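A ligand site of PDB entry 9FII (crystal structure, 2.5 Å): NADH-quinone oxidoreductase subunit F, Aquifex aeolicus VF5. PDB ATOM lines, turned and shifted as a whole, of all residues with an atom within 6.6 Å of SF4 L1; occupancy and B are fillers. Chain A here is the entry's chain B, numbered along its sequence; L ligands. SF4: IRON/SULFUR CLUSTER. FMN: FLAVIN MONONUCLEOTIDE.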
ATOM      1  N   ILE A 181     -13.391 -13.104  14.407  1.00  0.00           N
ATOM      2  CA  ILE A 181     -14.080 -12.033  15.115  1.00  0.00           C
ATOM      3  C   ILE A 181     -13.338 -10.714  14.906  1.00  0.00           C
ATOM      4  O   ILE A 181     -13.938  -9.660  15.055  1.00  0.00           O
ATOM      5  CB  ILE A 181     -14.285 -12.357  16.619  1.00  0.00           C
ATOM      6  CG1 ILE A 181     -15.333 -11.433  17.254  1.00  0.00           C
ATOM      7  CG2 ILE A 181     -12.982 -12.318  17.407  1.00  0.00           C
ATOM      8  CD1 ILE A 181     -16.742 -11.581  16.672  1.00  0.00           C
ATOM      9  N   GLY A 197      -8.851  -9.869  20.464  1.00  0.00           N
ATOM     10  CA  GLY A 197      -9.897  -9.355  19.596  1.00  0.00           C
ATOM     11  C   GLY A 197     -11.277  -9.549  20.218  1.00  0.00           C
ATOM     12  O   GLY A 197     -12.091 -10.326  19.729  1.00  0.00           O
ATOM     13  N   HIS A 198     -11.532  -8.806  21.306  1.00  0.00           N
ATOM     14  CA  HIS A 198     -12.807  -8.867  21.981  1.00  0.00           C
ATOM     15  C   HIS A 198     -13.667  -7.692  21.498  1.00  0.00           C
ATOM     16  O   HIS A 198     -13.301  -6.541  21.696  1.00  0.00           O
ATOM     17  CB  HIS A 198     -12.596  -8.877  23.499  1.00  0.00           C
ATOM     18  CG  HIS A 198     -12.097 -10.182  24.056  1.00  0.00           C
ATOM     19  ND1 HIS A 198     -11.308 -10.242  25.182  1.00  0.00           N
ATOM     20  CD2 HIS A 198     -12.310 -11.459  23.705  1.00  0.00           C
ATOM     21  CE1 HIS A 198     -11.020 -11.510  25.464  1.00  0.00           C
ATOM     22  NE2 HIS A 198     -11.645 -12.270  24.596  1.00  0.00           N
ATOM     23  N   PRO A 199     -14.808  -7.934  20.827  1.00  0.00           N
ATOM     24  CA  PRO A 199     -15.760  -6.861  20.547  1.00  0.00           C
ATOM     25  C   PRO A 199     -16.074  -6.008  21.776  1.00  0.00           C
ATOM     26  O   PRO A 199     -16.263  -6.549  22.872  1.00  0.00           O
ATOM     27  CB  PRO A 199     -16.975  -7.653  20.061  1.00  0.00           C
ATOM     28  CG  PRO A 199     -16.359  -8.825  19.331  1.00  0.00           C
ATOM     29  CD  PRO A 199     -15.211  -9.214  20.248  1.00  0.00           C
ATOM     30  N   ARG A 200     -16.032  -4.682  21.583  1.00  0.00           N
ATOM     31  CA  ARG A 200     -16.503  -3.693  22.531  1.00  0.00           C
ATOM     32  C   ARG A 200     -18.013  -3.559  22.465  1.00  0.00           C
ATOM     33  O   ARG A 200     -18.625  -3.726  21.420  1.00  0.00           O
ATOM     34  CB  ARG A 200     -15.978  -2.279  22.208  1.00  0.00           C
ATOM     35  CG  ARG A 200     -14.473  -2.129  22.315  1.00  0.00           C
ATOM     36  CD  ARG A 200     -14.053  -0.754  21.828  1.00  0.00           C
ATOM     37  NE  ARG A 200     -12.601  -0.603  21.845  1.00  0.00           N
ATOM     38  CZ  ARG A 200     -11.937   0.453  21.383  1.00  0.00           C
ATOM     39  NH1 ARG A 200     -12.598   1.466  20.867  1.00  0.00           N
ATOM     40  NH2 ARG A 200     -10.617   0.490  21.455  1.00  0.00           N
ATOM     41  N   GLU A 345     -14.824 -19.845  16.632  1.00  0.00           N
ATOM     42  CA  GLU A 345     -14.698 -18.423  16.364  1.00  0.00           C
ATOM     43  C   GLU A 345     -15.365 -17.527  17.423  1.00  0.00           C
ATOM     44  O   GLU A 345     -15.050 -16.331  17.480  1.00  0.00           O
ATOM     45  CB  GLU A 345     -15.248 -18.115  14.974  1.00  0.00           C
ATOM     46  CG  GLU A 345     -14.440 -18.755  13.844  1.00  0.00           C
ATOM     47  CD  GLU A 345     -12.941 -18.493  13.780  1.00  0.00           C
ATOM     48  OE1 GLU A 345     -12.417 -17.566  14.459  1.00  0.00           O
ATOM     49  OE2 GLU A 345     -12.300 -19.276  13.036  1.00  0.00           O
ATOM     50  N   THR A 346     -16.281 -18.061  18.244  1.00  0.00           N
ATOM     51  CA  THR A 346     -16.796 -17.305  19.363  1.00  0.00           C
ATOM     52  C   THR A 346     -15.619 -16.821  20.213  1.00  0.00           C
ATOM     53  O   THR A 346     -14.710 -17.606  20.504  1.00  0.00           O
ATOM     54  CB  THR A 346     -17.810 -18.093  20.190  1.00  0.00           C
ATOM     55  OG1 THR A 346     -18.235 -17.243  21.257  1.00  0.00           O
ATOM     56  CG2 THR A 346     -17.255 -19.381  20.790  1.00  0.00           C
ATOM     57  N   CYS A 347     -15.643 -15.545  20.608  1.00  0.00           N
ATOM     58  CA  CYS A 347     -14.562 -14.969  21.408  1.00  0.00           C
ATOM     59  C   CYS A 347     -14.713 -15.303  22.891  1.00  0.00           C
ATOM     60  O   CYS A 347     -13.737 -15.176  23.619  1.00  0.00           O
ATOM     61  CB  CYS A 347     -14.400 -13.471  21.198  1.00  0.00           C
ATOM     62  SG  CYS A 347     -15.558 -12.430  22.127  1.00  0.00           S
ATOM     63  N   GLY A 348     -15.943 -15.665  23.323  1.00  0.00           N
ATOM     64  CA  GLY A 348     -16.162 -16.259  24.643  1.00  0.00           C
ATOM     65  C   GLY A 348     -16.679 -15.268  25.700  1.00  0.00           C
ATOM     66  O   GLY A 348     -17.109 -15.692  26.758  1.00  0.00           O
ATOM     67  N   GLN A 349     -16.611 -13.965  25.408  1.00  0.00           N
ATOM     68  CA  GLN A 349     -17.005 -12.904  26.337  1.00  0.00           C
ATOM     69  C   GLN A 349     -18.400 -13.150  26.904  1.00  0.00           C
ATOM     70  O   GLN A 349     -18.600 -12.988  28.116  1.00  0.00           O
ATOM     71  CB  GLN A 349     -17.034 -11.539  25.646  1.00  0.00           C
ATOM     72  CG  GLN A 349     -15.793 -10.688  25.875  1.00  0.00           C
ATOM     73  CD  GLN A 349     -15.899  -9.312  25.221  1.00  0.00           C
ATOM     74  OE1 GLN A 349     -16.190  -9.185  24.027  1.00  0.00           O
ATOM     75  NE2 GLN A 349     -15.683  -8.277  26.015  1.00  0.00           N
ATOM     76  N   CYS A 350     -19.362 -13.470  26.027  1.00  0.00           N
ATOM     77  CA  CYS A 350     -20.767 -13.623  26.394  1.00  0.00           C
ATOM     78  C   CYS A 350     -21.041 -15.113  26.653  1.00  0.00           C
ATOM     79  O   CYS A 350     -20.545 -15.950  25.916  1.00  0.00           O
ATOM     80  CB  CYS A 350     -21.686 -13.083  25.308  1.00  0.00           C
ATOM     81  SG  CYS A 350     -21.103 -11.554  24.493  1.00  0.00           S
ATOM     82  N   THR A 351     -21.816 -15.427  27.696  1.00  0.00           N
ATOM     83  CA  THR A 351     -21.914 -16.797  28.164  1.00  0.00           C
ATOM     84  C   THR A 351     -22.730 -17.611  27.160  1.00  0.00           C
ATOM     85  O   THR A 351     -22.290 -18.677  26.701  1.00  0.00           O
ATOM     86  CB  THR A 351     -22.468 -16.863  29.583  1.00  0.00           C
ATOM     87  OG1 THR A 351     -21.411 -16.567  30.489  1.00  0.00           O
ATOM     88  CG2 THR A 351     -22.929 -18.261  29.973  1.00  0.00           C
ATOM     89  N   CYS A 353     -23.286 -17.262  23.958  1.00  0.00           N
ATOM     90  CA  CYS A 353     -22.521 -17.464  22.736  1.00  0.00           C
ATOM     91  C   CYS A 353     -21.439 -18.505  22.966  1.00  0.00           C
ATOM     92  O   CYS A 353     -21.309 -19.463  22.206  1.00  0.00           O
ATOM     93  CB  CYS A 353     -21.956 -16.133  22.253  1.00  0.00           C
ATOM     94  SG  CYS A 353     -20.941 -16.172  20.741  1.00  0.00           S
ATOM     95  N   ARG A 354     -20.648 -18.321  24.033  1.00  0.00           N
ATOM     96  CA  ARG A 354     -19.519 -19.177  24.327  1.00  0.00           C
ATOM     97  C   ARG A 354     -19.983 -20.632  24.403  1.00  0.00           C
ATOM     98  O   ARG A 354     -19.399 -21.508  23.787  1.00  0.00           O
ATOM     99  CB  ARG A 354     -18.904 -18.754  25.679  1.00  0.00           C
ATOM    100  CG  ARG A 354     -17.780 -19.624  26.218  1.00  0.00           C
ATOM    101  CD  ARG A 354     -17.145 -19.073  27.498  1.00  0.00           C
ATOM    102  NE  ARG A 354     -17.964 -19.289  28.694  1.00  0.00           N
ATOM    103  CZ  ARG A 354     -18.706 -18.368  29.315  1.00  0.00           C
ATOM    104  NH1 ARG A 354     -18.795 -17.133  28.837  1.00  0.00           N
ATOM    105  NH2 ARG A 354     -19.382 -18.699  30.391  1.00  0.00           N
ATOM    106  N   CYS A 357     -22.297 -21.972  21.189  1.00  0.00           N
ATOM    107  CA  CYS A 357     -21.558 -22.285  19.977  1.00  0.00           C
ATOM    108  C   CYS A 357     -20.818 -23.613  20.124  1.00  0.00           C
ATOM    109  O   CYS A 357     -20.717 -24.368  19.163  1.00  0.00           O
ATOM    110  CB  CYS A 357     -20.546 -21.203  19.610  1.00  0.00           C
ATOM    111  SG  CYS A 357     -21.259 -19.709  18.883  1.00  0.00           S
ATOM    112  N   ILE A 387     -28.330 -19.050  21.573  1.00  0.00           N
ATOM    113  CA  ILE A 387     -26.973 -18.549  21.452  1.00  0.00           C
ATOM    114  C   ILE A 387     -27.014 -17.036  21.584  1.00  0.00           C
ATOM    115  O   ILE A 387     -26.058 -16.438  22.073  1.00  0.00           O
ATOM    116  CB  ILE A 387     -26.330 -19.013  20.140  1.00  0.00           C
ATOM    117  CG1 ILE A 387     -26.356 -20.538  19.986  1.00  0.00           C
ATOM    118  CG2 ILE A 387     -24.901 -18.476  20.008  1.00  0.00           C
ATOM    119  CD1 ILE A 387     -25.838 -21.048  18.646  1.00  0.00           C
ATOM    120  N   GLN A 388     -28.128 -16.410  21.172  1.00  0.00           N
ATOM    121  CA  GLN A 388     -28.209 -14.961  20.987  1.00  0.00           C
ATOM    122  C   GLN A 388     -28.195 -14.180  22.315  1.00  0.00           C
ATOM    123  O   GLN A 388     -27.465 -13.180  22.420  1.00  0.00           O
ATOM    124  CB  GLN A 388     -29.482 -14.561  20.225  1.00  0.00           C
ATOM    125  CG  GLN A 388     -29.807 -13.076  20.345  1.00  0.00           C
ATOM    126  CD  GLN A 388     -30.797 -12.553  19.331  1.00  0.00           C
ATOM    127  OE1 GLN A 388     -30.535 -12.493  18.114  1.00  0.00           O
ATOM    128  NE2 GLN A 388     -31.961 -12.129  19.809  1.00  0.00           N
ATOM    129  N   THR A 390     -27.952 -11.829  25.485  1.00  0.00           N
ATOM    130  CA  THR A 390     -26.899 -11.133  26.221  1.00  0.00           C
ATOM    131  C   THR A 390     -25.680 -10.828  25.351  1.00  0.00           C
ATOM    132  O   THR A 390     -24.726 -10.253  25.866  1.00  0.00           O
ATOM    133  CB  THR A 390     -26.463 -11.876  27.487  1.00  0.00           C
ATOM    134  OG1 THR A 390     -25.604 -12.979  27.207  1.00  0.00           O
ATOM    135  CG2 THR A 390     -27.638 -12.344  28.323  1.00  0.00           C
ATOM    136  N   SER A 391     -25.673 -11.234  24.069  1.00  0.00           N
ATOM    137  CA  SER A 391     -24.497 -11.050  23.223  1.00  0.00           C
ATOM    138  C   SER A 391     -24.348  -9.589  22.822  1.00  0.00           C
ATOM    139  O   SER A 391     -25.341  -8.873  22.703  1.00  0.00           O
ATOM    140  CB  SER A 391     -24.521 -11.926  21.991  1.00  0.00           C
ATOM    141  OG  SER A 391     -25.788 -11.958  21.367  1.00  0.00           O
ATOM    142  N   ILE A 392     -23.109  -9.163  22.600  1.00  0.00           N
ATOM    143  CA  ILE A 392     -22.851  -7.757  22.363  1.00  0.00           C
ATOM    144  C   ILE A 392     -22.217  -7.567  20.987  1.00  0.00           C
ATOM    145  O   ILE A 392     -21.564  -6.561  20.778  1.00  0.00           O
ATOM    146  CB  ILE A 392     -22.046  -7.105  23.507  1.00  0.00           C
ATOM    147  CG1 ILE A 392     -20.909  -7.964  24.064  1.00  0.00           C
ATOM    148  CG2 ILE A 392     -23.007  -6.697  24.635  1.00  0.00           C
ATOM    149  CD1 ILE A 392     -19.538  -7.644  23.504  1.00  0.00           C
ATOM    150  N   CYS A 393     -22.493  -8.502  20.069  1.00  0.00           N
ATOM    151  CA  CYS A 393     -21.996  -8.451  18.706  1.00  0.00           C
ATOM    152  C   CYS A 393     -22.761  -9.462  17.845  1.00  0.00           C
ATOM    153  O   CYS A 393     -23.535 -10.276  18.348  1.00  0.00           O
ATOM    154  CB  CYS A 393     -20.490  -8.692  18.626  1.00  0.00           C
ATOM    155  SG  CYS A 393     -20.002 -10.344  18.069  1.00  0.00           S
ATOM    156  N   GLY A 394     -22.524  -9.412  16.541  1.00  0.00           N
ATOM    157  CA  GLY A 394     -23.417 -10.032  15.581  1.00  0.00           C
ATOM    158  C   GLY A 394     -23.207 -11.537  15.444  1.00  0.00           C
ATOM    159  O   GLY A 394     -24.091 -12.206  14.928  1.00  0.00           O
ATOM    160  N   LEU A 395     -22.047 -12.073  15.878  1.00  0.00           N
ATOM    161  CA  LEU A 395     -21.716 -13.487  15.696  1.00  0.00           C
ATOM    162  C   LEU A 395     -22.657 -14.355  16.538  1.00  0.00           C
ATOM    163  O   LEU A 395     -23.120 -15.410  16.073  1.00  0.00           O
ATOM    164  CB  LEU A 395     -20.256 -13.754  16.053  1.00  0.00           C
ATOM    165  CG  LEU A 395     -19.760 -15.191  15.866  1.00  0.00           C
ATOM    166  CD1 LEU A 395     -18.250 -15.280  15.674  1.00  0.00           C
ATOM    167  CD2 LEU A 395     -20.169 -16.040  17.058  1.00  0.00           C
ATOM    168  N   GLY A 396     -22.908 -13.920  17.774  1.00  0.00           N
ATOM    169  CA  GLY A 396     -23.882 -14.553  18.632  1.00  0.00           C
ATOM    170  C   GLY A 396     -25.286 -14.459  18.046  1.00  0.00           C
ATOM    171  O   GLY A 396     -26.055 -15.419  18.119  1.00  0.00           O
ATOM    172  N   ALA A 397     -25.622 -13.319  17.468  1.00  0.00           N
ATOM    173  CA  ALA A 397     -26.943 -13.111  16.867  1.00  0.00           C
ATOM    174  C   ALA A 397     -27.244 -14.136  15.758  1.00  0.00           C
ATOM    175  O   ALA A 397     -28.405 -14.469  15.597  1.00  0.00           O
ATOM    176  CB  ALA A 397     -27.057 -11.681  16.361  1.00  0.00           C
HETATM  177 FE1  SF4 L   1     -17.702 -12.696  21.509  1.00  0.00          FE
HETATM  178 FE2  SF4 L   1     -19.916 -14.160  20.868  1.00  0.00          FE
HETATM  179 FE3  SF4 L   1     -19.612 -11.689  19.903  1.00  0.00          FE
HETATM  180 FE4  SF4 L   1     -20.069 -12.044  22.549  1.00  0.00          FE
HETATM  181  S1  SF4 L   1     -21.483 -12.539  20.800  1.00  0.00           S
HETATM  182  S2  SF4 L   1     -18.576 -10.644  21.637  1.00  0.00           S
HETATM  183  S3  SF4 L   1     -18.931 -13.933  22.932  1.00  0.00           S
HETATM  184  S4  SF4 L   1     -18.325 -13.485  19.452  1.00  0.00           S
HETATM  185  N1  FMN L   2     -16.498  -6.418   7.751  1.00  0.00           N
HETATM  186  C2  FMN L   2     -15.505  -6.508   6.816  1.00  0.00           C
HETATM  187  O2  FMN L   2     -15.280  -5.578   6.037  1.00  0.00           O
HETATM  188  N3  FMN L   2     -14.730  -7.666   6.757  1.00  0.00           N
HETATM  189  C4  FMN L   2     -14.876  -8.791   7.546  1.00  0.00           C
HETATM  190  O4  FMN L   2     -14.158  -9.780   7.387  1.00  0.00           O
HETATM  191  C4A FMN L   2     -15.905  -8.690   8.540  1.00  0.00           C
HETATM  192  N5  FMN L   2     -16.061  -9.671   9.376  1.00  0.00           N
HETATM  193  C5A FMN L   2     -17.019  -9.534  10.358  1.00  0.00           C
HETATM  194  C6  FMN L   2     -17.142 -10.560  11.297  1.00  0.00           C
HETATM  195  C7  FMN L   2     -18.076 -10.484  12.319  1.00  0.00           C
HETATM  196  C7M FMN L   2     -18.147 -11.597  13.330  1.00  0.00           C
HETATM  197  C8  FMN L   2     -18.927  -9.369  12.408  1.00  0.00           C
HETATM  198  C8M FMN L   2     -20.010  -9.301  13.442  1.00  0.00           C
HETATM  199  C9  FMN L   2     -18.795  -8.341  11.484  1.00  0.00           C
HETATM  200  C9A FMN L   2     -17.839  -8.392  10.465  1.00  0.00           C
HETATM  201  N10 FMN L   2     -17.649  -7.330   9.547  1.00  0.00           N
HETATM  202  C10 FMN L   2     -16.684  -7.450   8.572  1.00  0.00           C
HETATM  203  C1' FMN L   2     -18.398  -6.084   9.621  1.00  0.00           C
HETATM  204  C2' FMN L   2     -17.588  -4.958  10.261  1.00  0.00           C
HETATM  205  O2' FMN L   2     -17.716  -4.973  11.683  1.00  0.00           O
HETATM  206  C3' FMN L   2     -17.991  -3.574   9.735  1.00  0.00           C
HETATM  207  O3' FMN L   2     -19.415  -3.450   9.645  1.00  0.00           O
HETATM  208  C4' FMN L   2     -17.405  -3.211   8.372  1.00  0.00           C
HETATM  209  O4' FMN L   2     -16.007  -3.478   8.362  1.00  0.00           O
HETATM  210  C5' FMN L   2     -17.664  -1.751   8.076  1.00  0.00           C
HETATM  211  O5' FMN L   2     -17.122  -1.386   6.799  1.00  0.00           O
HETATM  212  P   FMN L   2     -18.166  -1.049   5.599  1.00  0.00           P
HETATM  213  O1P FMN L   2     -19.084  -2.233   5.335  1.00  0.00           O
HETATM  214  O2P FMN L   2     -18.934   0.167   5.964  1.00  0.00           O
HETATM  215  O3P FMN L   2     -17.205  -0.783   4.405  1.00  0.00           O
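Residues that only touch SF4 L1: Ile 181 (3.7 Å), Pro 199 (3.7 Å), Ser 391 (3.3 Å), Ile 392 (3.7 Å) and Leu 395 (3.9 Å). Hydrophobic or aromatic side chains within 4 Å of SF4 L1: Ile 181, Pro 199, Ile 392 and Leu 395. Of the 25 residues printed, 13 come within 4 Å of SF4 L1. The nearest printed residue that does not touch SF4 L1 is Glu 345 (4.8 Å).
The backbone NH of Cys 347 lies close to a sulfur (S4) of SF4 L1 (3.6 Å). An iron atom (FE1) of SF4 L1 is bound by the side-chain sulfur of Cys 347 (2.2 Å). N of Cys 350 sits close to S3 of SF4 L1 (3.2 Å). An iron atom (FE4) of SF4 L1 is bound by the side-chain sulfur of Cys 350 (2.3 Å). An iron atom (FE2) of SF4 L1 is bound by the side-chain sulfur (SG) of Cys 353, 2.3 Å away. The side-chain sulfur (SG) of Cys 393 binds an iron atom (FE3) of SF4 L1. The backbone NH (N) of Gln 349 sits close to a sulfur (S3) of SF4 L1, 3.4 Å away. OE1 of Gln 349 sits close to S2 of SF4 L1 (3.7 Å). A sulfur (S3) of SF4 L1 sits close to the backbone NH of Gly 348 (3.5 Å). S3 of SF4 L1 sits close to OG1 of Thr 346, 3.8 Å away. N of Gly 396 lies close to S1 of SF4 L1 (3.6 Å).
The backbone NH of Gln 349 lies close to the side-chain sulfur of Cys 347, 3.8 Å away. N of Ile 392 sits close to SG of Cys 350 (3.7 Å). SG of Cys 357 sits close to O of Cys 353 (3.3 Å). The backbone NH (N) of Cys 353 sits at hydrogen-bond distance from the backbone carbonyl oxygen (O) of Ile 387 (3.5 Å). N of Leu 395 lies close to SG of Cys 393. The side-chain amide oxygen of Gln 349 lies close to the backbone carbonyl oxygen of Pro 199, 2.9 Å away. N of Gly 348 sits close to OG1 of Thr 346 (3.5 Å). The backbone carbonyl oxygen of Gly 348 sits at hydrogen-bond distance from the guanidinium group of Arg 354 (3.0 Å).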
